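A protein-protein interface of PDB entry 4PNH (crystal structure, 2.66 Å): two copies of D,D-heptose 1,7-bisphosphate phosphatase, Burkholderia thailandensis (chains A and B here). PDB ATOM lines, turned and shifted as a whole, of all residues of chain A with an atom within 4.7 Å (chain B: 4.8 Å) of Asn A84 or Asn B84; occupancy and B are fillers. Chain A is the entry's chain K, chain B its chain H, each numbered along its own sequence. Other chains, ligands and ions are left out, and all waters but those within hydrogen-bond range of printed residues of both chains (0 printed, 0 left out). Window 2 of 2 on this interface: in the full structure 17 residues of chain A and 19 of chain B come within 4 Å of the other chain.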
ATOM      1  N   MET A  80      -8.004 -15.930 -10.864  1.00  0.00           N
ATOM      2  CA  MET A  80      -9.263 -16.663 -10.835  1.00  0.00           C
ATOM      3  C   MET A  80      -9.480 -17.436 -12.128  1.00  0.00           C
ATOM      4  O   MET A  80     -10.108 -18.494 -12.125  1.00  0.00           O
ATOM      5  CB  MET A  80     -10.440 -15.716 -10.588  1.00  0.00           C
ATOM      6  CG  MET A  80     -10.736 -15.464  -9.118  1.00  0.00           C
ATOM      7  SD  MET A  80     -10.927 -16.965  -8.128  1.00  0.00           S
ATOM      8  CE  MET A  80     -12.158 -17.868  -9.068  1.00  0.00           C
ATOM      9  N   ALA A  81      -8.957 -16.903 -13.226  1.00  0.00           N
ATOM     10  CA  ALA A  81      -9.099 -17.527 -14.535  1.00  0.00           C
ATOM     11  C   ALA A  81      -8.526 -18.943 -14.561  1.00  0.00           C
ATOM     12  O   ALA A  81      -9.168 -19.865 -15.062  1.00  0.00           O
ATOM     13  CB  ALA A  81      -8.429 -16.674 -15.596  1.00  0.00           C
ATOM     14  N   THR A  82      -7.325 -19.112 -14.020  1.00  0.00           N
ATOM     15  CA  THR A  82      -6.689 -20.426 -13.968  1.00  0.00           C
ATOM     16  C   THR A  82      -7.504 -21.429 -13.151  1.00  0.00           C
ATOM     17  O   THR A  82      -7.655 -22.588 -13.540  1.00  0.00           O
ATOM     18  CB  THR A  82      -5.268 -20.330 -13.371  1.00  0.00           C
ATOM     19  OG1 THR A  82      -4.423 -19.596 -14.265  1.00  0.00           O
ATOM     20  CG2 THR A  82      -4.675 -21.717 -13.145  1.00  0.00           C
ATOM     21  N   LEU A  83      -8.044 -20.967 -12.031  1.00  0.00           N
ATOM     22  CA  LEU A  83      -8.825 -21.815 -11.138  1.00  0.00           C
ATOM     23  C   LEU A  83     -10.150 -22.278 -11.735  1.00  0.00           C
ATOM     24  O   LEU A  83     -10.529 -23.438 -11.588  1.00  0.00           O
ATOM     25  CB  LEU A  83      -9.086 -21.077  -9.827  1.00  0.00           C
ATOM     26  CG  LEU A  83      -8.338 -21.612  -8.608  1.00  0.00           C
ATOM     27  CD1 LEU A  83      -8.544 -20.686  -7.429  1.00  0.00           C
ATOM     28  CD2 LEU A  83      -8.820 -23.019  -8.282  1.00  0.00           C
ATOM     29  N   ASN A  84     -10.860 -21.363 -12.387  1.00  0.00           N
ATOM     30  CA  ASN A  84     -12.140 -21.692 -13.006  1.00  0.00           C
ATOM     31  C   ASN A  84     -11.991 -22.679 -14.159  1.00  0.00           C
ATOM     32  O   ASN A  84     -12.774 -23.621 -14.281  1.00  0.00           O
ATOM     33  CB  ASN A  84     -12.846 -20.423 -13.486  1.00  0.00           C
ATOM     34  CG  ASN A  84     -13.590 -19.712 -12.368  1.00  0.00           C
ATOM     35  OD1 ASN A  84     -14.333 -20.336 -11.608  1.00  0.00           O
ATOM     36  ND2 ASN A  84     -13.399 -18.402 -12.268  1.00  0.00           N
ATOM     37  N   ALA A  85     -10.987 -22.452 -15.002  1.00  0.00           N
ATOM     38  CA  ALA A  85     -10.710 -23.328 -16.134  1.00  0.00           C
ATOM     39  C   ALA A  85     -10.471 -24.758 -15.668  1.00  0.00           C
ATOM     40  O   ALA A  85     -10.920 -25.715 -16.301  1.00  0.00           O
ATOM     41  CB  ALA A  85      -9.509 -22.818 -16.915  1.00  0.00           C
ATOM     42  N   MET A  86      -9.750 -24.886 -14.558  1.00  0.00           N
ATOM     43  CA  MET A  86      -9.419 -26.186 -13.987  1.00  0.00           C
ATOM     44  C   MET A  86     -10.620 -26.926 -13.410  1.00  0.00           C
ATOM     45  O   MET A  86     -10.782 -28.124 -13.642  1.00  0.00           O
ATOM     46  CB  MET A  86      -8.368 -26.015 -12.891  1.00  0.00           C
ATOM     47  CG  MET A  86      -8.108 -27.275 -12.093  1.00  0.00           C
ATOM     48  SD  MET A  86      -7.025 -26.972 -10.691  1.00  0.00           S
ATOM     49  CE  MET A  86      -5.480 -26.639 -11.536  1.00  0.00           C
ATOM     50  N   HIS A  87     -11.475 -26.215 -12.681  1.00  0.00           N
ATOM     51  CA  HIS A  87     -12.648 -26.857 -12.104  1.00  0.00           C
ATOM     52  C   HIS A  87     -13.633 -27.205 -13.197  1.00  0.00           C
ATOM     53  O   HIS A  87     -14.314 -28.220 -13.115  1.00  0.00           O
ATOM     54  CB  HIS A  87     -13.323 -25.982 -11.047  1.00  0.00           C
ATOM     55  CG  HIS A  87     -14.526 -26.623 -10.420  1.00  0.00           C
ATOM     56  ND1 HIS A  87     -15.781 -26.050 -10.457  1.00  0.00           N
ATOM     57  CD2 HIS A  87     -14.671 -27.798  -9.768  1.00  0.00           C
ATOM     58  CE1 HIS A  87     -16.643 -26.840  -9.838  1.00  0.00           C
ATOM     59  NE2 HIS A  87     -15.994 -27.908  -9.411  1.00  0.00           N
ATOM     60  N   LEU A  88     -13.679 -26.378 -14.236  1.00  0.00           N
ATOM     61  CA  LEU A  88     -14.602 -26.603 -15.337  1.00  0.00           C
ATOM     62  C   LEU A  88     -14.137 -27.796 -16.158  1.00  0.00           C
ATOM     63  O   LEU A  88     -14.945 -28.633 -16.559  1.00  0.00           O
ATOM     64  CB  LEU A  88     -14.704 -25.356 -16.216  1.00  0.00           C
ATOM     65  CG  LEU A  88     -15.984 -25.151 -17.026  1.00  0.00           C
ATOM     66  CD1 LEU A  88     -17.218 -25.267 -16.142  1.00  0.00           C
ATOM     67  CD2 LEU A  88     -15.950 -23.808 -17.738  1.00  0.00           C
ATOM     68  N   MET B  80     -15.612 -24.084  -4.894  1.00  0.00           N
ATOM     69  CA  MET B  80     -15.391 -23.013  -5.865  1.00  0.00           C
ATOM     70  C   MET B  80     -16.323 -21.847  -5.573  1.00  0.00           C
ATOM     71  O   MET B  80     -15.998 -20.692  -5.853  1.00  0.00           O
ATOM     72  CB  MET B  80     -15.601 -23.512  -7.298  1.00  0.00           C
ATOM     73  CG  MET B  80     -14.361 -24.102  -7.963  1.00  0.00           C
ATOM     74  SD  MET B  80     -12.903 -23.027  -7.930  1.00  0.00           S
ATOM     75  CE  MET B  80     -13.558 -21.509  -8.623  1.00  0.00           C
ATOM     76  N   ALA B  81     -17.491 -22.163  -5.026  1.00  0.00           N
ATOM     77  CA  ALA B  81     -18.479 -21.153  -4.676  1.00  0.00           C
ATOM     78  C   ALA B  81     -17.927 -20.149  -3.662  1.00  0.00           C
ATOM     79  O   ALA B  81     -18.085 -18.939  -3.835  1.00  0.00           O
ATOM     80  CB  ALA B  81     -19.733 -21.817  -4.131  1.00  0.00           C
ATOM     81  N   THR B  82     -17.282 -20.648  -2.611  1.00  0.00           N
ATOM     82  CA  THR B  82     -16.694 -19.786  -1.587  1.00  0.00           C
ATOM     83  C   THR B  82     -15.619 -18.875  -2.178  1.00  0.00           C
ATOM     84  O   THR B  82     -15.526 -17.696  -1.836  1.00  0.00           O
ATOM     85  CB  THR B  82     -16.082 -20.612  -0.433  1.00  0.00           C
ATOM     86  OG1 THR B  82     -17.122 -21.297   0.276  1.00  0.00           O
ATOM     87  CG2 THR B  82     -15.324 -19.713   0.537  1.00  0.00           C
ATOM     88  N   LEU B  83     -14.820 -19.432  -3.078  1.00  0.00           N
ATOM     89  CA  LEU B  83     -13.736 -18.704  -3.723  1.00  0.00           C
ATOM     90  C   LEU B  83     -14.253 -17.597  -4.634  1.00  0.00           C
ATOM     91  O   LEU B  83     -13.711 -16.492  -4.650  1.00  0.00           O
ATOM     92  CB  LEU B  83     -12.862 -19.677  -4.514  1.00  0.00           C
ATOM     93  CG  LEU B  83     -11.468 -19.963  -3.955  1.00  0.00           C
ATOM     94  CD1 LEU B  83     -10.813 -21.077  -4.745  1.00  0.00           C
ATOM     95  CD2 LEU B  83     -10.618 -18.704  -3.999  1.00  0.00           C
ATOM     96  N   ASN B  84     -15.300 -17.904  -5.396  1.00  0.00           N
ATOM     97  CA  ASN B  84     -15.907 -16.944  -6.316  1.00  0.00           C
ATOM     98  C   ASN B  84     -16.528 -15.753  -5.600  1.00  0.00           C
ATOM     99  O   ASN B  84     -16.393 -14.613  -6.044  1.00  0.00           O
ATOM    100  CB  ASN B  84     -16.968 -17.627  -7.182  1.00  0.00           C
ATOM    101  CG  ASN B  84     -16.372 -18.355  -8.369  1.00  0.00           C
ATOM    102  OD1 ASN B  84     -15.539 -17.810  -9.090  1.00  0.00           O
ATOM    103  ND2 ASN B  84     -16.812 -19.589  -8.589  1.00  0.00           N
ATOM    104  N   ALA B  85     -17.222 -16.028  -4.502  1.00  0.00           N
ATOM    105  CA  ALA B  85     -17.861 -14.984  -3.708  1.00  0.00           C
ATOM    106  C   ALA B  85     -16.867 -13.928  -3.238  1.00  0.00           C
ATOM    107  O   ALA B  85     -17.169 -12.737  -3.243  1.00  0.00           O
ATOM    108  CB  ALA B  85     -18.571 -15.595  -2.511  1.00  0.00           C
ATOM    109  N   MET B  86     -15.687 -14.371  -2.816  1.00  0.00           N
ATOM    110  CA  MET B  86     -14.663 -13.455  -2.330  1.00  0.00           C
ATOM    111  C   MET B  86     -14.065 -12.586  -3.428  1.00  0.00           C
ATOM    112  O   MET B  86     -13.879 -11.387  -3.236  1.00  0.00           O
ATOM    113  CB  MET B  86     -13.545 -14.236  -1.641  1.00  0.00           C
ATOM    114  CG  MET B  86     -12.344 -13.389  -1.243  1.00  0.00           C
ATOM    115  SD  MET B  86     -10.981 -14.372  -0.590  1.00  0.00           S
ATOM    116  CE  MET B  86     -10.581 -15.354  -2.031  1.00  0.00           C
ATOM    117  N   HIS B  87     -13.794 -13.175  -4.590  1.00  0.00           N
ATOM    118  CA  HIS B  87     -13.203 -12.410  -5.682  1.00  0.00           C
ATOM    119  C   HIS B  87     -14.213 -11.397  -6.196  1.00  0.00           C
ATOM    120  O   HIS B  87     -13.841 -10.303  -6.606  1.00  0.00           O
ATOM    121  CB  HIS B  87     -12.734 -13.317  -6.819  1.00  0.00           C
ATOM    122  CG  HIS B  87     -12.073 -12.577  -7.940  1.00  0.00           C
ATOM    123  ND1 HIS B  87     -12.529 -12.620  -9.243  1.00  0.00           N
ATOM    124  CD2 HIS B  87     -10.990 -11.764  -7.953  1.00  0.00           C
ATOM    125  CE1 HIS B  87     -11.752 -11.875 -10.006  1.00  0.00           C
ATOM    126  NE2 HIS B  87     -10.809 -11.341  -9.245  1.00  0.00           N
ATOM    127  N   LEU B  88     -15.491 -11.760  -6.146  1.00  0.00           N
ATOM    128  CA  LEU B  88     -16.555 -10.873  -6.596  1.00  0.00           C
ATOM    129  C   LEU B  88     -16.772  -9.740  -5.604  1.00  0.00           C
ATOM    130  O   LEU B  88     -16.929  -8.582  -5.994  1.00  0.00           O
ATOM    131  CB  LEU B  88     -17.857 -11.656  -6.776  1.00  0.00           C
ATOM    132  CG  LEU B  88     -18.917 -11.111  -7.735  1.00  0.00           C
ATOM    133  CD1 LEU B  88     -18.323 -10.798  -9.100  1.00  0.00           C
ATOM    134  CD2 LEU B  88     -20.073 -12.090  -7.852  1.00  0.00           C
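The backbone carbonyl oxygen of Met B80 lies within hydrogen-bond range of the side-chain amide nitrogen of Asn B84, at 3.1 Å.
The side-chain amide nitrogen (ND2) of Asn A84 lies within hydrogen-bond range of the backbone carbonyl oxygen (O) of Met A80 (3.3 Å).
Met B80 touches Met A80 (CE to CE, 3.9 Å).
Met A80 touches Asn B84 (CE to OD1, 3.4 Å).
Met A80 touches His B87 (CG to ND1, 3.4 Å).
CD1 of Leu A83 touches CD1 of Leu B83 (3.5 Å).
Asn A84 touches Met B80 (OD1 to CE, 3.3 Å).
Asn B84 touches Asn A84 (OD1 to OD1, 3.8 Å).
His A87 touches Met B80 (ND1 to CG, 3.5 Å).
Of the printed residues of chain B, His A87 touches Met B80 (3.5 Å).
Of the printed residues of chain A, Met B80 touches Met A80 (3.9 Å), Asn A84 (3.3 Å) and His A87 (3.5 Å).
Printed residues of chain A within 4 Å of Asn B84: Met A80 (3.4 Å) and Asn A84 (3.8 Å).
The nearest printed residue of chain A that does not touch Asn B84 is His A87 (6.8 Å).
Of the 9 printed residues of chain B, 4 touch a printed residue of chain A.
Hydrophobic or aromatic side chains of chain B within 4 Å of the printed part of chain A: Met B80, Leu B83 and His B87.
Among the printed residues, no Asp or Glu carboxylate lies within 4 Å of a Lys or Arg side-chain nitrogen of the other chain.
Met B80 touches its own counterpart, Met A80.
Met A80 touches His B87, and with the chains exchanged His A87 touches Met B80.
Leu B83 touches its own counterpart, Leu A83.
Asn B84 touches its own counterpart, Asn A84.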
